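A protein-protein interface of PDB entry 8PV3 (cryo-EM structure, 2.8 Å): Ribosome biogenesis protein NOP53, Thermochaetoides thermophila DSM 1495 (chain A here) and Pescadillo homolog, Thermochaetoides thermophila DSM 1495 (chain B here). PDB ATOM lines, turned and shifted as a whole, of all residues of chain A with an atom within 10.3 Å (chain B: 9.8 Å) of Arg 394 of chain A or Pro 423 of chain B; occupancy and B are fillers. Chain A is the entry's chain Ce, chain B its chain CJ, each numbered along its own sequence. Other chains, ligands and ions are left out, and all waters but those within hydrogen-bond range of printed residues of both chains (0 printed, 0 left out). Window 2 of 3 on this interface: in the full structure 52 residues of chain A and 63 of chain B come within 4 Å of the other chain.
OD1 of Asn 216 of chain A touches CB of Leu 482 of chain B, at 3.5 Å. O of Asp 391 of chain A touches CD2 of Leu 482 of chain B (3.8 Å). CB of Ser 392 of chain A touches OD1 of Asp 421 of chain B, at 3.6 Å. Leu 393 of chain A touches Asp 421 of chain B (N to OD2, 3.6 Å). Arg 394 of chain A touches Pro 423 of chain B. Leu 396 of chain A touches Tyr 212 of chain B (CD2 to OH, 3.5 Å).
Of the 12 printed residues of chain A, 7 touch a printed residue of chain B. Hydrophobic or aromatic side chains of chain B within 4 Å of the printed part of chain A: Leu 190, Tyr 212, Pro 423 and Leu 482.
The backbone carbonyl oxygen (O) of Leu 190 of chain B lies within hydrogen-bond range of the backbone NH (N) of Tyr 215 of chain A, 3.1 Å away. The side-chain amide oxygen of Asn 216 of chain A lies close to the side-chain amide oxygen of Gln 459 of chain B. The side-chain carboxylate (OD2) of Asp 421 of chain B is in hydrogen-bond range of the backbone NH (N) of Arg 394 of chain A (3.0 Å). OE1 of Gln 459 of chain B lies close to OH of Tyr 215 of chain A (2.3 Å).
The backbone NH of Arg 394 of chain A sits close to the side-chain hydroxyl of Ser 392 of chain A (3.5 Å). The backbone NH (N) of Arg 395 of chain A lies within hydrogen-bond range of the side-chain hydroxyl (OG) of Ser 392 of chain A. The side-chain carboxylate (OE2) of Glu 377 of chain B lies within hydrogen-bond range of the backbone NH (N) of Asp 421 of chain B, 2.7 Å away. The side-chain amide oxygen (OE1) of Gln 457 of chain B sits close to the side-chain carboxylate (OD1) of Asp 421 of chain B, at 3.4 Å.
Leu 389 of chain A touches none of the printed residues of chain B. Glu 390 of chain A touches none of the printed residues of chain B. Ser 392 of chain A touches just one residue of chain B: Asp 421 (3.6 Å). Of the printed residues of chain B, Arg 394 of chain A touches Asp 421 (3.0 Å) and Pro 423 (3.996 Å). Printed residues of chain B within 4 Å of Leu 396 of chain A: Tyr 212 (3.5 Å). Printed residues of chain A within 4 Å of Leu 190 of chain B: Tyr 215 (3.1 Å). Of the printed residues of chain A, Pro 423 of chain B touches Arg 394. The nearest printed residue of chain B that does not touch Arg 394 of chain A is Glu 377 of chain B (4.2 Å). The nearest printed residue of chain B that does not touch Asn 216 of chain A is Leu 190 of chain B (5.0 Å).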
ATOM      1  N   TYR A 215      16.701 -12.454  -6.041  1.00  0.00           N
ATOM      2  CA  TYR A 215      17.881 -13.134  -5.518  1.00  0.00           C
ATOM      3  C   TYR A 215      18.358 -12.496  -4.221  1.00  0.00           C
ATOM      4  O   TYR A 215      18.997 -13.163  -3.400  1.00  0.00           O
ATOM      5  CB  TYR A 215      18.998 -13.133  -6.563  1.00  0.00           C
ATOM      6  CG  TYR A 215      19.923 -11.939  -6.498  1.00  0.00           C
ATOM      7  CD1 TYR A 215      19.521 -10.698  -6.968  1.00  0.00           C
ATOM      8  CD2 TYR A 215      21.207 -12.059  -5.982  1.00  0.00           C
ATOM      9  CE1 TYR A 215      20.364  -9.608  -6.913  1.00  0.00           C
ATOM     10  CE2 TYR A 215      22.056 -10.973  -5.925  1.00  0.00           C
ATOM     11  CZ  TYR A 215      21.629  -9.752  -6.391  1.00  0.00           C
ATOM     12  OH  TYR A 215      22.472  -8.669  -6.336  1.00  0.00           O
ATOM     13  N   ASN A 216      18.059 -11.214  -4.022  1.00  0.00           N
ATOM     14  CA  ASN A 216      18.382 -10.492  -2.795  1.00  0.00           C
ATOM     15  C   ASN A 216      17.086  -9.839  -2.336  1.00  0.00           C
ATOM     16  O   ASN A 216      16.894  -8.626  -2.491  1.00  0.00           O
ATOM     17  CB  ASN A 216      19.496  -9.472  -3.029  1.00  0.00           C
ATOM     18  CG  ASN A 216      19.889  -8.734  -1.773  1.00  0.00           C
ATOM     19  OD1 ASN A 216      20.382  -7.609  -1.827  1.00  0.00           O
ATOM     20  ND2 ASN A 216      19.675  -9.367  -0.627  1.00  0.00           N
ATOM     21  N   LEU A 389      20.817 -18.970   1.772  1.00  0.00           N
ATOM     22  CA  LEU A 389      21.030 -17.624   1.248  1.00  0.00           C
ATOM     23  C   LEU A 389      22.512 -17.325   1.090  1.00  0.00           C
ATOM     24  O   LEU A 389      23.330 -17.678   1.943  1.00  0.00           O
ATOM     25  CB  LEU A 389      20.387 -16.566   2.150  1.00  0.00           C
ATOM     26  CG  LEU A 389      18.939 -16.140   1.897  1.00  0.00           C
ATOM     27  CD1 LEU A 389      17.955 -17.199   2.291  1.00  0.00           C
ATOM     28  CD2 LEU A 389      18.638 -14.832   2.617  1.00  0.00           C
ATOM     29  N   GLU A 390      22.847 -16.672  -0.016  1.00  0.00           N
ATOM     30  CA  GLU A 390      24.191 -16.197  -0.293  1.00  0.00           C
ATOM     31  C   GLU A 390      24.176 -14.681  -0.435  1.00  0.00           C
ATOM     32  O   GLU A 390      23.137 -14.062  -0.679  1.00  0.00           O
ATOM     33  CB  GLU A 390      24.749 -16.859  -1.556  1.00  0.00           C
ATOM     34  CG  GLU A 390      24.882 -18.369  -1.448  1.00  0.00           C
ATOM     35  CD  GLU A 390      26.075 -18.798  -0.615  1.00  0.00           C
ATOM     36  OE1 GLU A 390      26.991 -17.975  -0.408  1.00  0.00           O
ATOM     37  OE2 GLU A 390      26.094 -19.963  -0.166  1.00  0.00           O
ATOM     38  N   ASP A 391      25.354 -14.082  -0.282  1.00  0.00           N
ATOM     39  CA  ASP A 391      25.484 -12.633  -0.230  1.00  0.00           C
ATOM     40  C   ASP A 391      25.936 -12.017  -1.546  1.00  0.00           C
ATOM     41  O   ASP A 391      26.140 -10.799  -1.603  1.00  0.00           O
ATOM     42  CB  ASP A 391      26.459 -12.235   0.883  1.00  0.00           C
ATOM     43  CG  ASP A 391      25.907 -12.515   2.265  1.00  0.00           C
ATOM     44  OD1 ASP A 391      24.670 -12.478   2.432  1.00  0.00           O
ATOM     45  OD2 ASP A 391      26.710 -12.774   3.188  1.00  0.00           O
ATOM     46  N   SER A 392      26.093 -12.809  -2.602  1.00  0.00           N
ATOM     47  CA  SER A 392      26.615 -12.314  -3.865  1.00  0.00           C
ATOM     48  C   SER A 392      25.852 -12.922  -5.031  1.00  0.00           C
ATOM     49  O   SER A 392      25.257 -13.997  -4.916  1.00  0.00           O
ATOM     50  CB  SER A 392      28.109 -12.628  -4.006  1.00  0.00           C
ATOM     51  OG  SER A 392      28.317 -14.009  -4.237  1.00  0.00           O
ATOM     52  N   LEU A 393      25.869 -12.207  -6.158  1.00  0.00           N
ATOM     53  CA  LEU A 393      25.308 -12.744  -7.393  1.00  0.00           C
ATOM     54  C   LEU A 393      26.143 -13.907  -7.912  1.00  0.00           C
ATOM     55  O   LEU A 393      25.625 -14.800  -8.591  1.00  0.00           O
ATOM     56  CB  LEU A 393      25.214 -11.639  -8.446  1.00  0.00           C
ATOM     57  CG  LEU A 393      24.489 -11.951  -9.757  1.00  0.00           C
ATOM     58  CD1 LEU A 393      23.080 -12.438  -9.492  1.00  0.00           C
ATOM     59  CD2 LEU A 393      24.477 -10.736 -10.663  1.00  0.00           C
ATOM     60  N   ARG A 394      27.444 -13.901  -7.610  1.00  0.00           N
ATOM     61  CA  ARG A 394      28.332 -14.973  -8.045  1.00  0.00           C
ATOM     62  C   ARG A 394      27.951 -16.305  -7.411  1.00  0.00           C
ATOM     63  O   ARG A 394      27.960 -17.347  -8.073  1.00  0.00           O
ATOM     64  CB  ARG A 394      29.776 -14.610  -7.703  1.00  0.00           C
ATOM     65  CG  ARG A 394      30.810 -15.587  -8.218  1.00  0.00           C
ATOM     66  CD  ARG A 394      32.192 -15.200  -7.729  1.00  0.00           C
ATOM     67  NE  ARG A 394      32.211 -15.016  -6.283  1.00  0.00           N
ATOM     68  CZ  ARG A 394      32.353 -15.999  -5.405  1.00  0.00           C
ATOM     69  NH1 ARG A 394      32.496 -17.256  -5.790  1.00  0.00           N
ATOM     70  NH2 ARG A 394      32.346 -15.713  -4.106  1.00  0.00           N
ATOM     71  N   ARG A 395      27.604 -16.286  -6.128  1.00  0.00           N
ATOM     72  CA  ARG A 395      27.246 -17.494  -5.399  1.00  0.00           C
ATOM     73  C   ARG A 395      25.760 -17.816  -5.474  1.00  0.00           C
ATOM     74  O   ARG A 395      25.279 -18.631  -4.682  1.00  0.00           O
ATOM     75  CB  ARG A 395      27.669 -17.374  -3.934  1.00  0.00           C
ATOM     76  CG  ARG A 395      29.160 -17.222  -3.724  1.00  0.00           C
ATOM     77  CD  ARG A 395      29.629 -18.079  -2.566  1.00  0.00           C
ATOM     78  NE  ARG A 395      29.259 -19.477  -2.750  1.00  0.00           N
ATOM     79  CZ  ARG A 395      29.500 -20.437  -1.870  1.00  0.00           C
ATOM     80  NH1 ARG A 395      30.106 -20.185  -0.721  1.00  0.00           N
ATOM     81  NH2 ARG A 395      29.126 -21.682  -2.148  1.00  0.00           N
ATOM     82  N   LEU A 396      25.027 -17.191  -6.392  1.00  0.00           N
ATOM     83  CA  LEU A 396      23.598 -17.446  -6.514  1.00  0.00           C
ATOM     84  C   LEU A 396      23.342 -18.866  -7.002  1.00  0.00           C
ATOM     85  O   LEU A 396      24.020 -19.364  -7.904  1.00  0.00           O
ATOM     86  CB  LEU A 396      22.960 -16.437  -7.470  1.00  0.00           C
ATOM     87  CG  LEU A 396      21.467 -16.593  -7.771  1.00  0.00           C
ATOM     88  CD1 LEU A 396      20.651 -16.567  -6.490  1.00  0.00           C
ATOM     89  CD2 LEU A 396      20.992 -15.516  -8.727  1.00  0.00           C
ATOM     90  N   LYS A 397      22.355 -19.517  -6.389  1.00  0.00           N
ATOM     91  CA  LYS A 397      21.917 -20.861  -6.752  1.00  0.00           C
ATOM     92  C   LYS A 397      20.632 -20.729  -7.557  1.00  0.00           C
ATOM     93  O   LYS A 397      19.576 -20.403  -6.994  1.00  0.00           O
ATOM     94  CB  LYS A 397      21.687 -21.708  -5.499  1.00  0.00           C
ATOM     95  CG  LYS A 397      21.436 -23.178  -5.760  1.00  0.00           C
ATOM     96  CD  LYS A 397      22.733 -23.903  -6.030  1.00  0.00           C
ATOM     97  CE  LYS A 397      23.628 -23.877  -4.800  1.00  0.00           C
ATOM     98  NZ  LYS A 397      23.053 -24.659  -3.673  1.00  0.00           N
ATOM     99  N   PRO A 398      20.669 -20.932  -8.874  1.00  0.00           N
ATOM    100  CA  PRO A 398      19.435 -20.867  -9.666  1.00  0.00           C
ATOM    101  C   PRO A 398      18.478 -21.990  -9.292  1.00  0.00           C
ATOM    102  O   PRO A 398      18.893 -23.110  -8.991  1.00  0.00           O
ATOM    103  CB  PRO A 398      19.927 -21.003 -11.112  1.00  0.00           C
ATOM    104  CG  PRO A 398      21.321 -21.514 -11.018  1.00  0.00           C
ATOM    105  CD  PRO A 398      21.869 -21.059  -9.714  1.00  0.00           C
ATOM    106  N   LEU B 190      16.692  -9.279 -11.335  1.00  0.00           N
ATOM    107  CA  LEU B 190      17.483 -10.474 -11.044  1.00  0.00           C
ATOM    108  C   LEU B 190      16.711 -11.342 -10.059  1.00  0.00           C
ATOM    109  O   LEU B 190      16.829 -11.172  -8.844  1.00  0.00           O
ATOM    110  CB  LEU B 190      18.847 -10.098 -10.478  1.00  0.00           C
ATOM    111  CG  LEU B 190      19.865  -9.422 -11.388  1.00  0.00           C
ATOM    112  CD1 LEU B 190      20.944  -8.760 -10.554  1.00  0.00           C
ATOM    113  CD2 LEU B 190      20.471 -10.447 -12.322  1.00  0.00           C
ATOM    114  N   TYR B 212      20.321 -17.635 -16.412  1.00  0.00           N
ATOM    115  CA  TYR B 212      21.726 -17.366 -16.154  1.00  0.00           C
ATOM    116  C   TYR B 212      22.580 -18.332 -16.963  1.00  0.00           C
ATOM    117  O   TYR B 212      22.184 -19.471 -17.225  1.00  0.00           O
ATOM    118  CB  TYR B 212      22.038 -17.508 -14.666  1.00  0.00           C
ATOM    119  CG  TYR B 212      21.367 -16.481 -13.788  1.00  0.00           C
ATOM    120  CD1 TYR B 212      21.801 -15.164 -13.771  1.00  0.00           C
ATOM    121  CD2 TYR B 212      20.307 -16.831 -12.963  1.00  0.00           C
ATOM    122  CE1 TYR B 212      21.192 -14.224 -12.966  1.00  0.00           C
ATOM    123  CE2 TYR B 212      19.694 -15.897 -12.156  1.00  0.00           C
ATOM    124  CZ  TYR B 212      20.140 -14.597 -12.162  1.00  0.00           C
ATOM    125  OH  TYR B 212      19.533 -13.663 -11.359  1.00  0.00           O
ATOM    126  N   LYS B 213      23.759 -17.871 -17.374  1.00  0.00           N
ATOM    127  CA  LYS B 213      24.605 -18.672 -18.254  1.00  0.00           C
ATOM    128  C   LYS B 213      25.221 -19.802 -17.444  1.00  0.00           C
ATOM    129  O   LYS B 213      26.288 -19.653 -16.847  1.00  0.00           O
ATOM    130  CB  LYS B 213      25.675 -17.814 -18.917  1.00  0.00           C
ATOM    131  CG  LYS B 213      26.109 -18.364 -20.264  1.00  0.00           C
ATOM    132  CD  LYS B 213      27.064 -17.438 -20.986  1.00  0.00           C
ATOM    133  CE  LYS B 213      27.316 -17.931 -22.401  1.00  0.00           C
ATOM    134  NZ  LYS B 213      28.321 -17.102 -23.119  1.00  0.00           N
ATOM    135  N   PHE B 214      24.533 -20.941 -17.427  1.00  0.00           N
ATOM    136  CA  PHE B 214      25.002 -22.142 -16.753  1.00  0.00           C
ATOM    137  C   PHE B 214      24.558 -23.338 -17.578  1.00  0.00           C
ATOM    138  O   PHE B 214      23.891 -23.195 -18.605  1.00  0.00           O
ATOM    139  CB  PHE B 214      24.462 -22.239 -15.324  1.00  0.00           C
ATOM    140  CG  PHE B 214      25.034 -21.220 -14.388  1.00  0.00           C
ATOM    141  CD1 PHE B 214      26.365 -21.267 -14.024  1.00  0.00           C
ATOM    142  CD2 PHE B 214      24.237 -20.220 -13.863  1.00  0.00           C
ATOM    143  CE1 PHE B 214      26.896 -20.332 -13.162  1.00  0.00           C
ATOM    144  CE2 PHE B 214      24.761 -19.281 -12.998  1.00  0.00           C
ATOM    145  CZ  PHE B 214      26.092 -19.338 -12.649  1.00  0.00           C
ATOM    146  N   SER B 375      34.695  -7.267 -14.715  1.00  0.00           N
ATOM    147  CA  SER B 375      35.693  -8.258 -14.353  1.00  0.00           C
ATOM    148  C   SER B 375      35.302  -9.636 -14.874  1.00  0.00           C
ATOM    149  O   SER B 375      34.261  -9.826 -15.505  1.00  0.00           O
ATOM    150  CB  SER B 375      35.894  -8.307 -12.843  1.00  0.00           C
ATOM    151  OG  SER B 375      36.536  -7.130 -12.396  1.00  0.00           O
ATOM    152  N   ARG B 376      36.169 -10.607 -14.585  1.00  0.00           N
ATOM    153  CA  ARG B 376      36.034 -11.940 -15.157  1.00  0.00           C
ATOM    154  C   ARG B 376      34.826 -12.679 -14.591  1.00  0.00           C
ATOM    155  O   ARG B 376      34.177 -13.460 -15.295  1.00  0.00           O
ATOM    156  CB  ARG B 376      37.326 -12.717 -14.909  1.00  0.00           C
ATOM    157  CG  ARG B 376      37.378 -14.092 -15.513  1.00  0.00           C
ATOM    158  CD  ARG B 376      38.770 -14.673 -15.393  1.00  0.00           C
ATOM    159  NE  ARG B 376      39.201 -14.821 -14.009  1.00  0.00           N
ATOM    160  CZ  ARG B 376      40.224 -14.175 -13.469  1.00  0.00           C
ATOM    161  NH1 ARG B 376      40.949 -13.320 -14.171  1.00  0.00           N
ATOM    162  NH2 ARG B 376      40.530 -14.394 -12.194  1.00  0.00           N
ATOM    163  N   GLU B 377      34.494 -12.427 -13.325  1.00  0.00           N
ATOM    164  CA  GLU B 377      33.414 -13.171 -12.682  1.00  0.00           C
ATOM    165  C   GLU B 377      32.050 -12.569 -13.000  1.00  0.00           C
ATOM    166  O   GLU B 377      31.014 -13.183 -12.719  1.00  0.00           O
ATOM    167  CB  GLU B 377      33.642 -13.206 -11.173  1.00  0.00           C
ATOM    168  CG  GLU B 377      33.498 -11.849 -10.502  1.00  0.00           C
ATOM    169  CD  GLU B 377      34.776 -11.028 -10.519  1.00  0.00           C
ATOM    170  OE1 GLU B 377      35.745 -11.428 -11.199  1.00  0.00           O
ATOM    171  OE2 GLU B 377      34.812  -9.977  -9.848  1.00  0.00           O
ATOM    172  N   THR B 378      32.028 -11.371 -13.573  1.00  0.00           N
ATOM    173  CA  THR B 378      30.775 -10.668 -13.802  1.00  0.00           C
ATOM    174  C   THR B 378      30.050 -11.225 -15.030  1.00  0.00           C
ATOM    175  O   THR B 378      30.688 -11.689 -15.979  1.00  0.00           O
ATOM    176  CB  THR B 378      31.041  -9.179 -13.986  1.00  0.00           C
ATOM    177  OG1 THR B 378      31.750  -8.968 -15.213  1.00  0.00           O
ATOM    178  CG2 THR B 378      31.877  -8.662 -12.836  1.00  0.00           C
ATOM    179  N   PRO B 379      28.703 -11.191 -15.039  1.00  0.00           N
ATOM    180  CA  PRO B 379      27.969 -11.694 -16.209  1.00  0.00           C
ATOM    181  C   PRO B 379      27.983 -10.720 -17.380  1.00  0.00           C
ATOM    182  O   PRO B 379      27.255  -9.712 -17.410  1.00  0.00           O
ATOM    183  CB  PRO B 379      26.557 -11.925 -15.664  1.00  0.00           C
ATOM    184  CG  PRO B 379      26.429 -11.012 -14.510  1.00  0.00           C
ATOM    185  CD  PRO B 379      27.799 -10.769 -13.953  1.00  0.00           C
ATOM    186  N   ILE B 420      32.980  -5.713  -9.921  1.00  0.00           N
ATOM    187  CA  ILE B 420      33.641  -6.891  -9.366  1.00  0.00           C
ATOM    188  C   ILE B 420      32.656  -7.620  -8.462  1.00  0.00           C
ATOM    189  O   ILE B 420      31.690  -7.020  -7.978  1.00  0.00           O
ATOM    190  CB  ILE B 420      34.924  -6.537  -8.586  1.00  0.00           C
ATOM    191  CG1 ILE B 420      34.619  -5.649  -7.386  1.00  0.00           C
ATOM    192  CG2 ILE B 420      35.955  -5.860  -9.473  1.00  0.00           C
ATOM    193  CD1 ILE B 420      35.815  -5.487  -6.483  1.00  0.00           C
ATOM    194  N   ASP B 421      32.899  -8.912  -8.245  1.00  0.00           N
ATOM    195  CA  ASP B 421      32.086  -9.729  -7.353  1.00  0.00           C
ATOM    196  C   ASP B 421      32.914 -10.698  -6.517  1.00  0.00           C
ATOM    197  O   ASP B 421      32.355 -11.648  -5.956  1.00  0.00           O
ATOM    198  CB  ASP B 421      31.031 -10.497  -8.151  1.00  0.00           C
ATOM    199  CG  ASP B 421      29.735 -10.676  -7.386  1.00  0.00           C
ATOM    200  OD1 ASP B 421      29.671 -10.256  -6.212  1.00  0.00           O
ATOM    201  OD2 ASP B 421      28.780 -11.243  -7.958  1.00  0.00           O
ATOM    202  N   ARG B 422      34.224 -10.490  -6.415  1.00  0.00           N
ATOM    203  CA  ARG B 422      35.078 -11.372  -5.637  1.00  0.00           C
ATOM    204  C   ARG B 422      35.243 -10.833  -4.227  1.00  0.00           C
ATOM    205  O   ARG B 422      35.212  -9.610  -4.035  1.00  0.00           O
ATOM    206  CB  ARG B 422      36.454 -11.523  -6.301  1.00  0.00           C
ATOM    207  CG  ARG B 422      36.404 -12.132  -7.688  1.00  0.00           C
ATOM    208  CD  ARG B 422      37.748 -12.044  -8.391  1.00  0.00           C
ATOM    209  NE  ARG B 422      38.585 -13.203  -8.111  1.00  0.00           N
ATOM    210  CZ  ARG B 422      38.617 -14.299  -8.857  1.00  0.00           C
ATOM    211  NH1 ARG B 422      37.876 -14.416  -9.947  1.00  0.00           N
ATOM    212  NH2 ARG B 422      39.414 -15.302  -8.501  1.00  0.00           N
ATOM    213  N   PRO B 423      35.413 -11.698  -3.214  1.00  0.00           N
ATOM    214  CA  PRO B 423      35.630 -11.223  -1.845  1.00  0.00           C
ATOM    215  C   PRO B 423      37.026 -10.639  -1.644  1.00  0.00           C
ATOM    216  O   PRO B 423      37.139  -9.512  -1.162  1.00  0.00           O
ATOM    217  CB  PRO B 423      35.444 -12.486  -1.002  1.00  0.00           C
ATOM    218  CG  PRO B 423      35.783 -13.602  -1.922  1.00  0.00           C
ATOM    219  CD  PRO B 423      35.314 -13.168  -3.278  1.00  0.00           C
ATOM    220  N   ARG B 449      43.550  -1.562  -5.267  1.00  0.00           N
ATOM    221  CA  ARG B 449      42.520  -0.626  -5.701  1.00  0.00           C
ATOM    222  C   ARG B 449      43.179   0.551  -6.405  1.00  0.00           C
ATOM    223  O   ARG B 449      44.025   1.236  -5.820  1.00  0.00           O
ATOM    224  CB  ARG B 449      41.685  -0.147  -4.514  1.00  0.00           C
ATOM    225  CG  ARG B 449      40.347   0.453  -4.900  1.00  0.00           C
ATOM    226  CD  ARG B 449      39.518   0.805  -3.678  1.00  0.00           C
ATOM    227  NE  ARG B 449      38.541  -0.234  -3.378  1.00  0.00           N
ATOM    228  CZ  ARG B 449      38.487  -0.907  -2.236  1.00  0.00           C
ATOM    229  NH1 ARG B 449      39.344  -0.674  -1.256  1.00  0.00           N
ATOM    230  NH2 ARG B 449      37.550  -1.837  -2.074  1.00  0.00           N
ATOM    231  N   TYR B 455      34.532   1.054  -7.587  1.00  0.00           N
ATOM    232  CA  TYR B 455      34.196  -0.364  -7.613  1.00  0.00           C
ATOM    233  C   TYR B 455      32.768  -0.535  -7.119  1.00  0.00           C
ATOM    234  O   TYR B 455      32.446  -0.131  -5.997  1.00  0.00           O
ATOM    235  CB  TYR B 455      35.145  -1.186  -6.740  1.00  0.00           C
ATOM    236  CG  TYR B 455      36.561  -1.318  -7.248  1.00  0.00           C
ATOM    237  CD1 TYR B 455      36.902  -0.926  -8.531  1.00  0.00           C
ATOM    238  CD2 TYR B 455      37.548  -1.873  -6.448  1.00  0.00           C
ATOM    239  CE1 TYR B 455      38.192  -1.059  -8.993  1.00  0.00           C
ATOM    240  CE2 TYR B 455      38.842  -2.015  -6.905  1.00  0.00           C
ATOM    241  CZ  TYR B 455      39.158  -1.603  -8.178  1.00  0.00           C
ATOM    242  OH  TYR B 455      40.447  -1.737  -8.640  1.00  0.00           O
ATOM    243  N   GLN B 457      29.303  -3.437  -7.116  1.00  0.00           N
ATOM    244  CA  GLN B 457      28.768  -4.753  -7.407  1.00  0.00           C
ATOM    245  C   GLN B 457      27.727  -4.655  -8.525  1.00  0.00           C
ATOM    246  O   GLN B 457      27.203  -3.571  -8.791  1.00  0.00           O
ATOM    247  CB  GLN B 457      28.171  -5.360  -6.139  1.00  0.00           C
ATOM    248  CG  GLN B 457      29.168  -5.465  -5.003  1.00  0.00           C
ATOM    249  CD  GLN B 457      28.862  -6.609  -4.063  1.00  0.00           C
ATOM    250  OE1 GLN B 457      28.343  -7.643  -4.477  1.00  0.00           O
ATOM    251  NE2 GLN B 457      29.185  -6.430  -2.789  1.00  0.00           N
ATOM    252  N   PRO B 458      27.439  -5.769  -9.219  1.00  0.00           N
ATOM    253  CA  PRO B 458      26.522  -5.690 -10.375  1.00  0.00           C
ATOM    254  C   PRO B 458      25.103  -5.243 -10.049  1.00  0.00           C
ATOM    255  O   PRO B 458      24.403  -4.768 -10.949  1.00  0.00           O
ATOM    256  CB  PRO B 458      26.535  -7.122 -10.936  1.00  0.00           C
ATOM    257  CG  PRO B 458      27.301  -7.948  -9.963  1.00  0.00           C
ATOM    258  CD  PRO B 458      28.198  -7.030  -9.228  1.00  0.00           C
ATOM    259  N   GLN B 459      24.659  -5.366  -8.796  1.00  0.00           N
ATOM    260  CA  GLN B 459      23.307  -4.965  -8.412  1.00  0.00           C
ATOM    261  C   GLN B 459      23.111  -3.456  -8.536  1.00  0.00           C
ATOM    262  O   GLN B 459      21.980  -2.975  -8.675  1.00  0.00           O
ATOM    263  CB  GLN B 459      23.007  -5.429  -6.982  1.00  0.00           C
ATOM    264  CG  GLN B 459      21.548  -5.305  -6.570  1.00  0.00           C
ATOM    265  CD  GLN B 459      21.268  -5.908  -5.217  1.00  0.00           C
ATOM    266  OE1 GLN B 459      21.773  -6.979  -4.886  1.00  0.00           O
ATOM    267  NE2 GLN B 459      20.465  -5.219  -4.419  1.00  0.00           N
ATOM    268  N   ALA B 477      29.616  -1.162  -2.143  1.00  0.00           N
ATOM    269  CA  ALA B 477      31.048  -1.355  -2.031  1.00  0.00           C
ATOM    270  C   ALA B 477      31.389  -2.844  -2.027  1.00  0.00           C
ATOM    271  O   ALA B 477      30.554  -3.677  -1.666  1.00  0.00           O
ATOM    272  CB  ALA B 477      31.563  -0.688  -0.756  1.00  0.00           C
ATOM    273  N   PRO B 478      32.596  -3.203  -2.463  1.00  0.00           N
ATOM    274  CA  PRO B 478      33.013  -4.610  -2.415  1.00  0.00           C
ATOM    275  C   PRO B 478      33.079  -5.135  -0.989  1.00  0.00           C
ATOM    276  O   PRO B 478      33.630  -4.492  -0.094  1.00  0.00           O
ATOM    277  CB  PRO B 478      34.399  -4.586  -3.066  1.00  0.00           C
ATOM    278  CG  PRO B 478      34.387  -3.383  -3.918  1.00  0.00           C
ATOM    279  CD  PRO B 478      33.554  -2.375  -3.217  1.00  0.00           C
ATOM    280  N   GLY B 479      32.506  -6.318  -0.782  1.00  0.00           N
ATOM    281  CA  GLY B 479      32.466  -6.938   0.522  1.00  0.00           C
ATOM    282  C   GLY B 479      31.344  -6.470   1.420  1.00  0.00           C
ATOM    283  O   GLY B 479      31.108  -7.090   2.464  1.00  0.00           O
ATOM    284  N   ALA B 480      30.643  -5.402   1.051  1.00  0.00           N
ATOM    285  CA  ALA B 480      29.546  -4.898   1.858  1.00  0.00           C
ATOM    286  C   ALA B 480      28.258  -5.651   1.541  1.00  0.00           C
ATOM    287  O   ALA B 480      28.071  -6.183   0.444  1.00  0.00           O
ATOM    288  CB  ALA B 480      29.348  -3.400   1.624  1.00  0.00           C
ATOM    289  N   LEU B 482      24.456  -6.047   0.544  1.00  0.00           N
ATOM    290  CA  LEU B 482      23.768  -5.302  -0.495  1.00  0.00           C
ATOM    291  C   LEU B 482      22.423  -4.785   0.012  1.00  0.00           C
ATOM    292  O   LEU B 482      21.818  -5.381   0.907  1.00  0.00           O
ATOM    293  CB  LEU B 482      23.542  -6.177  -1.727  1.00  0.00           C
ATOM    294  CG  LEU B 482      24.643  -6.354  -2.778  1.00  0.00           C
ATOM    295  CD1 LEU B 482      25.013  -5.013  -3.389  1.00  0.00           C
ATOM    296  CD2 LEU B 482      25.871  -7.076  -2.243  1.00  0.00           C
